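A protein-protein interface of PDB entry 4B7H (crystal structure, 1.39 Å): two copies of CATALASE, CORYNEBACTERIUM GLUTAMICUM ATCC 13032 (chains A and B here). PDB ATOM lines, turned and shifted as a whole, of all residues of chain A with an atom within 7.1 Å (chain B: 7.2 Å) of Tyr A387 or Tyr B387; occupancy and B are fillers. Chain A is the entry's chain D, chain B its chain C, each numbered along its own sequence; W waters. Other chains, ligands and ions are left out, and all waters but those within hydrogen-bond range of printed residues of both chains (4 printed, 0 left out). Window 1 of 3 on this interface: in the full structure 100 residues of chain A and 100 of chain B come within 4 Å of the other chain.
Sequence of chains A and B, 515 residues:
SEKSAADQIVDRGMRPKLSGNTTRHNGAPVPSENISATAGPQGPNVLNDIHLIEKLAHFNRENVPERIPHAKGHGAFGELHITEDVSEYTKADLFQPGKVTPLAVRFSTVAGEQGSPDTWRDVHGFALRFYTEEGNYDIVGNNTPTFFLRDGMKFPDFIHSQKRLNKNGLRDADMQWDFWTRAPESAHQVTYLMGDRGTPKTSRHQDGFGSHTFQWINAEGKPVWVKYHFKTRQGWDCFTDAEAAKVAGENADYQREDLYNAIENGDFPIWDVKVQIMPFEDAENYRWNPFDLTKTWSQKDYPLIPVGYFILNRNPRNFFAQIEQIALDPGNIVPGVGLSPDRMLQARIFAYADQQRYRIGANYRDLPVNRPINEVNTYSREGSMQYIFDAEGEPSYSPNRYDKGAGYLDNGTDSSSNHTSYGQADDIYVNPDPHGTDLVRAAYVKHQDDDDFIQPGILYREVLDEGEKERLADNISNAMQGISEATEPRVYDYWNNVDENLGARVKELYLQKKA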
ATOM      1  N   ARG A  12      -3.818 -26.040 -25.076  1.00  0.00           N
ATOM      2  CA  ARG A  12      -3.259 -24.914 -24.326  1.00  0.00           C
ATOM      3  C   ARG A  12      -2.842 -23.776 -25.256  1.00  0.00           C
ATOM      4  O   ARG A  12      -2.095 -23.989 -26.213  1.00  0.00           O
ATOM      5  CB  ARG A  12      -2.019 -25.343 -23.543  1.00  0.00           C
ATOM      6  CG  ARG A  12      -2.203 -26.420 -22.509  1.00  0.00           C
ATOM      7  CD  ARG A  12      -0.815 -26.858 -22.057  1.00  0.00           C
ATOM      8  NE  ARG A  12      -0.825 -27.699 -20.868  1.00  0.00           N
ATOM      9  CZ  ARG A  12       0.265 -28.232 -20.325  1.00  0.00           C
ATOM     10  NH1 ARG A  12       1.456 -28.020 -20.871  1.00  0.00           N
ATOM     11  NH2 ARG A  12       0.165 -28.979 -19.238  1.00  0.00           N
ATOM     12  N   GLY A  13      -3.317 -22.566 -24.968  1.00  0.00           N
ATOM     13  CA  GLY A  13      -2.882 -21.385 -25.701  1.00  0.00           C
ATOM     14  C   GLY A  13      -3.682 -21.070 -26.956  1.00  0.00           C
ATOM     15  O   GLY A  13      -3.466 -20.036 -27.596  1.00  0.00           O
ATOM     16  N   MET A  14      -4.612 -21.954 -27.317  1.00  0.00           N
ATOM     17  CA  MET A  14      -5.358 -21.793 -28.560  1.00  0.00           C
ATOM     18  C   MET A  14      -6.589 -20.887 -28.406  1.00  0.00           C
ATOM     19  O   MET A  14      -7.421 -21.090 -27.513  1.00  0.00           O
ATOM     20  CB  MET A  14      -5.784 -23.158 -29.108  1.00  0.00           C
ATOM     21  CG  MET A  14      -6.380 -23.088 -30.506  1.00  0.00           C
ATOM     22  SD  MET A  14      -6.571 -24.689 -31.317  1.00  0.00           S
ATOM     23  CE  MET A  14      -7.753 -25.483 -30.235  1.00  0.00           C
ATOM     24  N   ALA A 321       3.930 -22.952 -33.178  1.00  0.00           N
ATOM     25  CA  ALA A 321       3.759 -22.759 -31.745  1.00  0.00           C
ATOM     26  C   ALA A 321       4.077 -24.009 -30.941  1.00  0.00           C
ATOM     27  O   ALA A 321       4.576 -23.914 -29.820  1.00  0.00           O
ATOM     28  CB  ALA A 321       2.352 -22.294 -31.450  1.00  0.00           C
ATOM     29  N   GLN A 325       8.603 -24.445 -31.611  1.00  0.00           N
ATOM     30  CA  GLN A 325       8.917 -23.971 -30.268  1.00  0.00           C
ATOM     31  C   GLN A 325       9.026 -25.061 -29.204  1.00  0.00           C
ATOM     32  O   GLN A 325       9.279 -24.747 -28.040  1.00  0.00           O
ATOM     33  CB  GLN A 325       7.867 -22.965 -29.806  1.00  0.00           C
ATOM     34  CG  GLN A 325       7.853 -21.692 -30.595  1.00  0.00           C
ATOM     35  CD  GLN A 325       6.984 -20.627 -29.957  1.00  0.00           C
ATOM     36  OE1 GLN A 325       7.353 -19.447 -29.922  1.00  0.00           O
ATOM     37  NE2 GLN A 325       5.814 -21.033 -29.456  1.00  0.00           N
ATOM     38  N   ASN A 363      12.397 -17.723 -20.796  1.00  0.00           N
ATOM     39  CA  ASN A 363      11.176 -18.299 -20.233  1.00  0.00           C
ATOM     40  C   ASN A 363      10.494 -19.339 -21.111  1.00  0.00           C
ATOM     41  O   ASN A 363       9.299 -19.603 -20.968  1.00  0.00           O
ATOM     42  CB  ASN A 363      10.231 -17.180 -19.785  1.00  0.00           C
ATOM     43  CG  ASN A 363      10.689 -16.568 -18.479  1.00  0.00           C
ATOM     44  OD1 ASN A 363      11.055 -17.301 -17.563  1.00  0.00           O
ATOM     45  ND2 ASN A 363      10.698 -15.238 -18.385  1.00  0.00           N
ATOM     46  N   ASP A 366       7.853 -21.942 -20.035  1.00  0.00           N
ATOM     47  CA  ASP A 366       6.489 -21.547 -19.725  1.00  0.00           C
ATOM     48  C   ASP A 366       5.545 -21.624 -20.924  1.00  0.00           C
ATOM     49  O   ASP A 366       4.322 -21.490 -20.773  1.00  0.00           O
ATOM     50  CB  ASP A 366       6.469 -20.136 -19.130  1.00  0.00           C
ATOM     51  CG  ASP A 366       7.169 -20.056 -17.776  1.00  0.00           C
ATOM     52  OD1 ASP A 366       7.101 -21.038 -17.011  1.00  0.00           O
ATOM     53  OD2 ASP A 366       7.789 -19.014 -17.479  1.00  0.00           O
ATOM     54  N   LEU A 367       6.095 -21.819 -22.122  1.00  0.00           N
ATOM     55  CA  LEU A 367       5.246 -21.952 -23.302  1.00  0.00           C
ATOM     56  C   LEU A 367       4.373 -23.201 -23.158  1.00  0.00           C
ATOM     57  O   LEU A 367       4.815 -24.197 -22.593  1.00  0.00           O
ATOM     58  CB  LEU A 367       6.070 -22.042 -24.580  1.00  0.00           C
ATOM     59  CG  LEU A 367       6.839 -20.779 -24.949  1.00  0.00           C
ATOM     60  CD1 LEU A 367       7.699 -21.060 -26.170  1.00  0.00           C
ATOM     61  CD2 LEU A 367       5.904 -19.607 -25.187  1.00  0.00           C
ATOM     62  N   PRO A 368       3.123 -23.138 -23.647  1.00  0.00           N
ATOM     63  CA  PRO A 368       2.162 -24.237 -23.519  1.00  0.00           C
ATOM     64  C   PRO A 368       2.742 -25.630 -23.771  1.00  0.00           C
ATOM     65  O   PRO A 368       2.547 -26.517 -22.944  1.00  0.00           O
ATOM     66  CB  PRO A 368       1.117 -23.877 -24.567  1.00  0.00           C
ATOM     67  CG  PRO A 368       1.053 -22.384 -24.469  1.00  0.00           C
ATOM     68  CD  PRO A 368       2.490 -21.941 -24.235  1.00  0.00           C
ATOM     69  N   ARG A 371       5.383 -26.749 -20.834  1.00  0.00           N
ATOM     70  CA  ARG A 371       4.983 -26.857 -19.437  1.00  0.00           C
ATOM     71  C   ARG A 371       4.606 -28.285 -19.115  1.00  0.00           C
ATOM     72  O   ARG A 371       3.947 -28.937 -19.922  1.00  0.00           O
ATOM     73  CB  ARG A 371       3.752 -25.995 -19.159  1.00  0.00           C
ATOM     74  CG  ARG A 371       3.944 -24.514 -19.314  1.00  0.00           C
ATOM     75  CD  ARG A 371       2.872 -23.775 -18.524  1.00  0.00           C
ATOM     76  NE  ARG A 371       1.502 -23.957 -19.013  1.00  0.00           N
ATOM     77  CZ  ARG A 371       0.912 -23.150 -19.892  1.00  0.00           C
ATOM     78  NH1 ARG A 371       1.575 -22.129 -20.409  1.00  0.00           N
ATOM     79  NH2 ARG A 371      -0.344 -23.364 -20.267  1.00  0.00           N
ATOM     80  N   GLU A 382      11.260 -13.600 -13.079  1.00  0.00           N
ATOM     81  CA  GLU A 382      11.574 -12.550 -14.054  1.00  0.00           C
ATOM     82  C   GLU A 382      12.065 -13.124 -15.386  1.00  0.00           C
ATOM     83  O   GLU A 382      11.603 -14.194 -15.809  1.00  0.00           O
ATOM     84  CB  GLU A 382      12.514 -11.500 -13.433  1.00  0.00           C
ATOM     85  CG  GLU A 382      11.876 -10.932 -12.147  1.00  0.00           C
ATOM     86  CD  GLU A 382      12.685  -9.874 -11.423  1.00  0.00           C
ATOM     87  OE1 GLU A 382      13.753  -9.462 -11.927  1.00  0.00           O
ATOM     88  OE2 GLU A 382      12.241  -9.457 -10.319  1.00  0.00           O
ATOM     89  N   GLY A 383      12.957 -12.408 -16.065  1.00  0.00           N
ATOM     90  CA  GLY A 383      13.326 -12.761 -17.426  1.00  0.00           C
ATOM     91  C   GLY A 383      12.354 -12.225 -18.463  1.00  0.00           C
ATOM     92  O   GLY A 383      11.190 -11.935 -18.159  1.00  0.00           O
ATOM     93  N   SER A 384      12.836 -12.118 -19.701  1.00  0.00           N
ATOM     94  CA  SER A 384      12.027 -11.647 -20.827  1.00  0.00           C
ATOM     95  C   SER A 384      10.732 -12.435 -20.967  1.00  0.00           C
ATOM     96  O   SER A 384      10.726 -13.656 -20.815  1.00  0.00           O
ATOM     97  CB  SER A 384      12.803 -11.775 -22.138  1.00  0.00           C
ATOM     98  OG  SER A 384      13.959 -10.969 -22.121  1.00  0.00           O
ATOM     99  N   MET A 385       9.637 -11.738 -21.264  1.00  0.00           N
ATOM    100  CA  MET A 385       8.376 -12.404 -21.586  1.00  0.00           C
ATOM    101  C   MET A 385       7.929 -13.372 -20.487  1.00  0.00           C
ATOM    102  O   MET A 385       7.583 -14.530 -20.755  1.00  0.00           O
ATOM    103  CB  MET A 385       8.488 -13.119 -22.942  1.00  0.00           C
ATOM    104  CG  MET A 385       8.588 -12.151 -24.126  1.00  0.00           C
ATOM    105  SD  MET A 385       7.039 -11.293 -24.461  1.00  0.00           S
ATOM    106  CE  MET A 385       6.031 -12.637 -25.049  1.00  0.00           C
ATOM    107  N   GLN A 386       7.950 -12.900 -19.245  1.00  0.00           N
ATOM    108  CA  GLN A 386       7.439 -13.704 -18.146  1.00  0.00           C
ATOM    109  C   GLN A 386       5.909 -13.723 -18.186  1.00  0.00           C
ATOM    110  O   GLN A 386       5.256 -12.719 -17.891  1.00  0.00           O
ATOM    111  CB  GLN A 386       7.932 -13.198 -16.783  1.00  0.00           C
ATOM    112  CG  GLN A 386       7.442 -14.103 -15.648  1.00  0.00           C
ATOM    113  CD  GLN A 386       7.793 -13.649 -14.246  1.00  0.00           C
ATOM    114  OE1 GLN A 386       8.264 -12.533 -14.023  1.00  0.00           O
ATOM    115  NE2 GLN A 386       7.549 -14.523 -13.287  1.00  0.00           N
ATOM    116  N   TYR A 387       5.345 -14.862 -18.582  1.00  0.00           N
ATOM    117  CA  TYR A 387       3.889 -14.993 -18.614  1.00  0.00           C
ATOM    118  C   TYR A 387       3.372 -15.493 -17.284  1.00  0.00           C
ATOM    119  O   TYR A 387       2.390 -14.961 -16.765  1.00  0.00           O
ATOM    120  CB  TYR A 387       3.438 -15.945 -19.715  1.00  0.00           C
ATOM    121  CG  TYR A 387       1.936 -16.024 -19.934  1.00  0.00           C
ATOM    122  CD1 TYR A 387       1.079 -16.538 -18.955  1.00  0.00           C
ATOM    123  CD2 TYR A 387       1.381 -15.615 -21.135  1.00  0.00           C
ATOM    124  CE1 TYR A 387      -0.279 -16.616 -19.165  1.00  0.00           C
ATOM    125  CE2 TYR A 387       0.023 -15.710 -21.360  1.00  0.00           C
ATOM    126  CZ  TYR A 387      -0.799 -16.202 -20.377  1.00  0.00           C
ATOM    127  OH  TYR A 387      -2.156 -16.273 -20.607  1.00  0.00           O
ATOM    128  N   ILE A 388       4.032 -16.492 -16.718  1.00  0.00           N
ATOM    129  CA  ILE A 388       3.579 -17.128 -15.488  1.00  0.00           C
ATOM    130  C   ILE A 388       4.390 -16.625 -14.303  1.00  0.00           C
ATOM    131  O   ILE A 388       5.614 -16.517 -14.382  1.00  0.00           O
ATOM    132  CB  ILE A 388       3.739 -18.653 -15.597  1.00  0.00           C
ATOM    133  CG1 ILE A 388       2.973 -19.174 -16.811  1.00  0.00           C
ATOM    134  CG2 ILE A 388       3.292 -19.334 -14.326  1.00  0.00           C
ATOM    135  CD1 ILE A 388       3.243 -20.625 -17.108  1.00  0.00           C
ATOM    136  N   PHE A 389       3.708 -16.291 -13.212  1.00  0.00           N
ATOM    137  CA  PHE A 389       4.394 -15.852 -12.001  1.00  0.00           C
ATOM    138  C   PHE A 389       3.785 -16.485 -10.757  1.00  0.00           C
ATOM    139  O   PHE A 389       2.629 -16.931 -10.770  1.00  0.00           O
ATOM    140  CB  PHE A 389       4.387 -14.323 -11.872  1.00  0.00           C
ATOM    141  CG  PHE A 389       3.011 -13.712 -11.957  1.00  0.00           C
ATOM    142  CD1 PHE A 389       2.478 -13.341 -13.183  1.00  0.00           C
ATOM    143  CD2 PHE A 389       2.242 -13.522 -10.813  1.00  0.00           C
ATOM    144  CE1 PHE A 389       1.202 -12.784 -13.274  1.00  0.00           C
ATOM    145  CE2 PHE A 389       0.969 -12.964 -10.898  1.00  0.00           C
ATOM    146  CZ  PHE A 389       0.452 -12.592 -12.132  1.00  0.00           C
ATOM    147  N   ARG B  12      -4.592 -13.028 -14.028  1.00  0.00           N
ATOM    148  CA  ARG B  12      -4.086 -13.729 -15.206  1.00  0.00           C
ATOM    149  C   ARG B  12      -2.620 -14.112 -15.029  1.00  0.00           C
ATOM    150  O   ARG B  12      -1.779 -13.260 -14.721  1.00  0.00           O
ATOM    151  CB  ARG B  12      -4.186 -12.844 -16.447  1.00  0.00           C
ATOM    152  CG  ARG B  12      -5.584 -12.502 -16.938  1.00  0.00           C
ATOM    153  CD  ARG B  12      -5.422 -11.399 -17.984  1.00  0.00           C
ATOM    154  NE  ARG B  12      -6.652 -11.011 -18.662  1.00  0.00           N
ATOM    155  CZ  ARG B  12      -6.714 -10.070 -19.600  1.00  0.00           C
ATOM    156  NH1 ARG B  12      -5.620  -9.410 -19.956  1.00  0.00           N
ATOM    157  NH2 ARG B  12      -7.871  -9.782 -20.179  1.00  0.00           N
ATOM    158  N   GLY B  13      -2.312 -15.390 -15.222  1.00  0.00           N
ATOM    159  CA  GLY B  13      -0.930 -15.838 -15.207  1.00  0.00           C
ATOM    160  C   GLY B  13      -0.389 -16.243 -13.849  1.00  0.00           C
ATOM    161  O   GLY B  13       0.733 -16.744 -13.764  1.00  0.00           O
ATOM    162  N   MET B  14      -1.173 -16.040 -12.790  1.00  0.00           N
ATOM    163  CA  MET B  14      -0.692 -16.302 -11.438  1.00  0.00           C
ATOM    164  C   MET B  14      -0.885 -17.758 -11.024  1.00  0.00           C
ATOM    165  O   MET B  14      -2.000 -18.286 -11.108  1.00  0.00           O
ATOM    166  CB  MET B  14      -1.400 -15.394 -10.441  1.00  0.00           C
ATOM    167  CG  MET B  14      -0.837 -15.476  -9.033  1.00  0.00           C
ATOM    168  SD  MET B  14      -1.390 -14.157  -7.948  1.00  0.00           S
ATOM    169  CE  MET B  14      -3.157 -14.447  -7.915  1.00  0.00           C
ATOM    170  N   ALA B 321       6.183  -8.730 -13.378  1.00  0.00           N
ATOM    171  CA  ALA B 321       5.348  -9.330 -14.410  1.00  0.00           C
ATOM    172  C   ALA B 321       4.282  -8.370 -14.918  1.00  0.00           C
ATOM    173  O   ALA B 321       3.919  -8.412 -16.093  1.00  0.00           O
ATOM    174  CB  ALA B 321       4.706 -10.599 -13.889  1.00  0.00           C
ATOM    175  N   GLN B 325       6.724  -5.097 -17.077  1.00  0.00           N
ATOM    176  CA  GLN B 325       6.357  -5.613 -18.397  1.00  0.00           C
ATOM    177  C   GLN B 325       5.104  -4.983 -19.003  1.00  0.00           C
ATOM    178  O   GLN B 325       4.730  -5.334 -20.121  1.00  0.00           O
ATOM    179  CB  GLN B 325       6.154  -7.129 -18.341  1.00  0.00           C
ATOM    180  CG  GLN B 325       7.422  -7.918 -18.043  1.00  0.00           C
ATOM    181  CD  GLN B 325       7.231  -9.413 -18.237  1.00  0.00           C
ATOM    182  OE1 GLN B 325       8.103 -10.093 -18.785  1.00  0.00           O
ATOM    183  NE2 GLN B 325       6.092  -9.935 -17.782  1.00  0.00           N
ATOM    184  N   ASN B 363       6.187 -10.582 -29.142  1.00  0.00           N
ATOM    185  CA  ASN B 363       4.867 -11.016 -28.683  1.00  0.00           C
ATOM    186  C   ASN B 363       4.427 -10.426 -27.353  1.00  0.00           C
ATOM    187  O   ASN B 363       3.589 -11.003 -26.651  1.00  0.00           O
ATOM    188  CB  ASN B 363       4.773 -12.542 -28.710  1.00  0.00           C
ATOM    189  CG  ASN B 363       4.583 -13.060 -30.122  1.00  0.00           C
ATOM    190  OD1 ASN B 363       3.769 -12.509 -30.868  1.00  0.00           O
ATOM    191  ND2 ASN B 363       5.345 -14.078 -30.517  1.00  0.00           N
ATOM    192  N   ASP B 366       0.808 -10.327 -25.938  1.00  0.00           N
ATOM    193  CA  ASP B 366       0.163 -11.522 -25.422  1.00  0.00           C
ATOM    194  C   ASP B 366       0.372 -11.732 -23.923  1.00  0.00           C
ATOM    195  O   ASP B 366      -0.281 -12.584 -23.323  1.00  0.00           O
ATOM    196  CB  ASP B 366       0.624 -12.742 -26.214  1.00  0.00           C
ATOM    197  CG  ASP B 366       0.215 -12.674 -27.689  1.00  0.00           C
ATOM    198  OD1 ASP B 366      -0.860 -12.117 -27.995  1.00  0.00           O
ATOM    199  OD2 ASP B 366       0.972 -13.179 -28.539  1.00  0.00           O
ATOM    200  N   LEU B 367       1.260 -10.955 -23.301  1.00  0.00           N
ATOM    201  CA  LEU B 367       1.451 -11.071 -21.853  1.00  0.00           C
ATOM    202  C   LEU B 367       0.169 -10.672 -21.139  1.00  0.00           C
ATOM    203  O   LEU B 367      -0.558  -9.788 -21.608  1.00  0.00           O
ATOM    204  CB  LEU B 367       2.597 -10.192 -21.371  1.00  0.00           C
ATOM    205  CG  LEU B 367       3.977 -10.572 -21.907  1.00  0.00           C
ATOM    206  CD1 LEU B 367       4.999  -9.547 -21.441  1.00  0.00           C
ATOM    207  CD2 LEU B 367       4.378 -11.966 -21.459  1.00  0.00           C
ATOM    208  N   PRO B 368      -0.132 -11.343 -20.023  1.00  0.00           N
ATOM    209  CA  PRO B 368      -1.359 -11.090 -19.260  1.00  0.00           C
ATOM    210  C   PRO B 368      -1.757  -9.615 -19.119  1.00  0.00           C
ATOM    211  O   PRO B 368      -2.897  -9.270 -19.438  1.00  0.00           O
ATOM    212  CB  PRO B 368      -1.037 -11.719 -17.903  1.00  0.00           C
ATOM    213  CG  PRO B 368      -0.223 -12.932 -18.286  1.00  0.00           C
ATOM    214  CD  PRO B 368       0.631 -12.480 -19.470  1.00  0.00           C
ATOM    215  N   ARG B 371      -2.872  -7.956 -22.699  1.00  0.00           N
ATOM    216  CA  ARG B 371      -4.001  -8.447 -23.487  1.00  0.00           C
ATOM    217  C   ARG B 371      -5.254  -7.682 -23.126  1.00  0.00           C
ATOM    218  O   ARG B 371      -5.507  -7.423 -21.948  1.00  0.00           O
ATOM    219  CB  ARG B 371      -4.270  -9.922 -23.200  1.00  0.00           C
ATOM    220  CG  ARG B 371      -3.123 -10.834 -23.465  1.00  0.00           C
ATOM    221  CD  ARG B 371      -3.639 -12.248 -23.629  1.00  0.00           C
ATOM    222  NE  ARG B 371      -4.243 -12.810 -22.423  1.00  0.00           N
ATOM    223  CZ  ARG B 371      -3.573 -13.548 -21.541  1.00  0.00           C
ATOM    224  NH1 ARG B 371      -2.285 -13.783 -21.727  1.00  0.00           N
ATOM    225  NH2 ARG B 371      -4.188 -14.049 -20.473  1.00  0.00           N
ATOM    226  N   GLU B 382       3.381 -16.251 -35.261  1.00  0.00           N
ATOM    227  CA  GLU B 382       4.766 -16.619 -34.990  1.00  0.00           C
ATOM    228  C   GLU B 382       5.495 -15.579 -34.149  1.00  0.00           C
ATOM    229  O   GLU B 382       4.873 -14.936 -33.308  1.00  0.00           O
ATOM    230  CB  GLU B 382       5.489 -16.983 -36.301  1.00  0.00           C
ATOM    231  CG  GLU B 382       4.733 -18.114 -37.009  1.00  0.00           C
ATOM    232  CD  GLU B 382       5.354 -18.623 -38.304  1.00  0.00           C
ATOM    233  OE1 GLU B 382       6.476 -18.209 -38.666  1.00  0.00           O
ATOM    234  OE2 GLU B 382       4.694 -19.465 -38.955  1.00  0.00           O
ATOM    235  N   GLY B 383       6.802 -15.437 -34.344  1.00  0.00           N
ATOM    236  CA  GLY B 383       7.606 -14.598 -33.471  1.00  0.00           C
ATOM    237  C   GLY B 383       8.055 -15.326 -32.212  1.00  0.00           C
ATOM    238  O   GLY B 383       7.468 -16.338 -31.798  1.00  0.00           O
ATOM    239  N   SER B 384       9.110 -14.803 -31.597  1.00  0.00           N
ATOM    240  CA  SER B 384       9.671 -15.385 -30.378  1.00  0.00           C
ATOM    241  C   SER B 384       8.617 -15.540 -29.291  1.00  0.00           C
ATOM    242  O   SER B 384       7.773 -14.665 -29.108  1.00  0.00           O
ATOM    243  CB  SER B 384      10.775 -14.487 -29.824  1.00  0.00           C
ATOM    244  OG  SER B 384      11.885 -14.406 -30.696  1.00  0.00           O
ATOM    245  N   MET B 385       8.669 -16.652 -28.563  1.00  0.00           N
ATOM    246  CA  MET B 385       7.821 -16.824 -27.389  1.00  0.00           C
ATOM    247  C   MET B 385       6.342 -16.621 -27.705  1.00  0.00           C
ATOM    248  O   MET B 385       5.632 -15.886 -27.009  1.00  0.00           O
ATOM    249  CB  MET B 385       8.278 -15.871 -26.276  1.00  0.00           C
ATOM    250  CG  MET B 385       9.622 -16.264 -25.660  1.00  0.00           C
ATOM    251  SD  MET B 385       9.556 -17.782 -24.680  1.00  0.00           S
ATOM    252  CE  MET B 385       8.572 -17.265 -23.288  1.00  0.00           C
ATOM    253  N   GLN B 386       5.873 -17.288 -28.756  1.00  0.00           N
ATOM    254  CA  GLN B 386       4.458 -17.240 -29.084  1.00  0.00           C
ATOM    255  C   GLN B 386       3.678 -18.126 -28.121  1.00  0.00           C
ATOM    256  O   GLN B 386       3.760 -19.351 -28.195  1.00  0.00           O
ATOM    257  CB  GLN B 386       4.186 -17.659 -30.536  1.00  0.00           C
ATOM    258  CG  GLN B 386       2.690 -17.603 -30.851  1.00  0.00           C
ATOM    259  CD  GLN B 386       2.311 -18.031 -32.259  1.00  0.00           C
ATOM    260  OE1 GLN B 386       3.087 -18.675 -32.973  1.00  0.00           O
ATOM    261  NE2 GLN B 386       1.092 -17.688 -32.659  1.00  0.00           N
ATOM    262  N   TYR B 387       2.954 -17.503 -27.194  1.00  0.00           N
ATOM    263  CA  TYR B 387       2.139 -18.279 -26.254  1.00  0.00           C
ATOM    264  C   TYR B 387       0.763 -18.528 -26.820  1.00  0.00           C
ATOM    265  O   TYR B 387       0.238 -19.635 -26.697  1.00  0.00           O
ATOM    266  CB  TYR B 387       1.988 -17.575 -24.912  1.00  0.00           C
ATOM    267  CG  TYR B 387       1.290 -18.379 -23.821  1.00  0.00           C
ATOM    268  CD1 TYR B 387      -0.050 -18.774 -23.938  1.00  0.00           C
ATOM    269  CD2 TYR B 387       1.961 -18.706 -22.657  1.00  0.00           C
ATOM    270  CE1 TYR B 387      -0.674 -19.495 -22.945  1.00  0.00           C
ATOM    271  CE2 TYR B 387       1.334 -19.398 -21.644  1.00  0.00           C
ATOM    272  CZ  TYR B 387       0.029 -19.800 -21.791  1.00  0.00           C
ATOM    273  OH  TYR B 387      -0.560 -20.513 -20.770  1.00  0.00           O
ATOM    274  N   ILE B 388       0.182 -17.526 -27.458  1.00  0.00           N
ATOM    275  CA  ILE B 388      -1.189 -17.611 -27.936  1.00  0.00           C
ATOM    276  C   ILE B 388      -1.212 -17.789 -29.445  1.00  0.00           C
ATOM    277  O   ILE B 388      -0.480 -17.113 -30.165  1.00  0.00           O
ATOM    278  CB  ILE B 388      -1.965 -16.335 -27.553  1.00  0.00           C
ATOM    279  CG1 ILE B 388      -1.942 -16.156 -26.032  1.00  0.00           C
ATOM    280  CG2 ILE B 388      -3.382 -16.378 -28.103  1.00  0.00           C
ATOM    281  CD1 ILE B 388      -2.484 -14.823 -25.570  1.00  0.00           C
ATOM    282  N   PHE B 389      -2.042 -18.710 -29.927  1.00  0.00           N
ATOM    283  CA  PHE B 389      -2.147 -18.934 -31.362  1.00  0.00           C
ATOM    284  C   PHE B 389      -3.603 -19.124 -31.774  1.00  0.00           C
ATOM    285  O   PHE B 389      -4.450 -19.484 -30.949  1.00  0.00           O
ATOM    286  CB  PHE B 389      -1.280 -20.126 -31.807  1.00  0.00           C
ATOM    287  CG  PHE B 389      -1.567 -21.400 -31.064  1.00  0.00           C
ATOM    288  CD1 PHE B 389      -2.559 -22.269 -31.509  1.00  0.00           C
ATOM    289  CD2 PHE B 389      -0.847 -21.730 -29.916  1.00  0.00           C
ATOM    290  CE1 PHE B 389      -2.822 -23.445 -30.828  1.00  0.00           C
ATOM    291  CE2 PHE B 389      -1.115 -22.896 -29.219  1.00  0.00           C
ATOM    292  CZ  PHE B 389      -2.106 -23.756 -29.678  1.00  0.00           C
HETATM  293  O   HOH W   1      10.041 -18.780 -30.058  1.00  0.00           O
HETATM  294  O   HOH W   2       9.937  -8.955 -20.500  1.00  0.00           O
HETATM  295  O   HOH W   3      11.722 -15.541 -22.510  1.00  0.00           O
HETATM  296  O   HOH W   4      -2.866 -18.993 -19.952  1.00  0.00           O
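O of Ala A321 is in hydrogen-bond range of NE2 of Gln A325, 3.2 Å away.
The backbone carbonyl oxygen (O) of Asp A366 sits at hydrogen-bond distance from the guanidinium group (NH1) of Arg A371, 2.8 Å away.
Of the printed residues of chain A, Asn B363 touches Met A385 (3.3 Å).
Printed residues of chain A within 4 Å of Leu B367: Met A385 (3.9 Å) and Gln A386 (3.8 Å).
The nearest printed residue of chain B that does not touch Met A385 is Ser B384 (4.9 Å).
The backbone carbonyl oxygen of Gly B13 lies within hydrogen-bond range of the backbone NH of Phe A389 (3.1 Å).
The side-chain amide oxygen (OE1) of Gln B325 lies within hydrogen-bond range of the backbone NH (N) of Met A385 (3.3 Å).
The side-chain amide oxygen (OE1) of Gln B325 sits at hydrogen-bond distance from the backbone NH (N) of Gln A386 (2.8 Å).
The guanidinium group (NH1) of Arg B371 lies within hydrogen-bond range of the side-chain hydroxyl (OH) of Tyr A387, 2.7 Å away.
The backbone NH of Met B385 sits at hydrogen-bond distance from the side-chain amide oxygen of Gln A325, 3.4 Å away.
The side-chain amide oxygen (OE1) of Gln A325 lies within hydrogen-bond range of the backbone NH (N) of Gln B386 (2.9 Å).
NH1 of Arg A371 sits at hydrogen-bond distance from OH of Tyr B387, 2.7 Å away.
O of Gly A13 is in hydrogen-bond range of N of Phe B389, 3.0 Å away.
Water W1 lies within hydrogen-bond range of OE1 of Gln A325 (2.8 Å) and N of Met B385 (2.9 Å).
Water W4 bridges OH of Tyr B387 and OH of Tyr A387.
Hydrophobic or aromatic side chains of chain A within 4 Å of the printed part of chain B: Met A14, Ala A321, Leu A367, Pro A368, Met A385, Tyr A387, Ile A388 and Phe A389.
Along chain B the printed residues that touch a printed residue of chain A span positions 12 to 389.
Among the printed residues, 33 pairs touch across the chains.
Among the printed residues, pairs that only touch across the chains: Arg A12 with Phe B389 (3.3 Å), Gly A13 with Tyr B387 (3.7 Å), Gly A13 with Ile B388 (3.3 Å), Met A14 with Phe B389 (3.4 Å), Ala A321 with Gln B386 (3.99 Å), Ala A321 with Phe B389 (3.6 Å), Gln A325 with Gly B383 (3.6 Å), Asn A363 with Met B385 (3.4 Å), Asp A366 with Tyr B387 (3.8 Å), Leu A367 with Met B385 (3.9 Å), Leu A367 with Gln B386 (3.7 Å), Pro A368 with Tyr B387 (3.6 Å), Gly A383 with Gln B325 (3.6 Å), Met A385 with Asn B363 (3.3 Å), Met A385 with Leu B367 (3.9 Å), Met A385 with Met B385 (3.8 Å), Gln A386 with Leu B367 (3.8 Å), Tyr A387 with Gly B13 (3.8 Å), Tyr A387 with Asp B366 (3.7 Å), Tyr A387 with Pro B368 (3.6 Å), Tyr A387 with Tyr B387 (3.5 Å), Ile A388 with Gly B13 (3.3 Å), Phe A389 with Arg B12 (3.3 Å), Phe A389 with Met B14 (3.4 Å) and Phe A389 with Ala B321 (3.6 Å).
Arg A12 touches Phe B389, and with the chains exchanged Phe A389 touches Arg B12.
Gly A13 touches Phe B389, and with the chains exchanged Phe A389 touches Gly B13.
Ala A321 touches Gln B386, but with the chains exchanged Gln A386 does not touch Ala B321 (4.1 Å).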
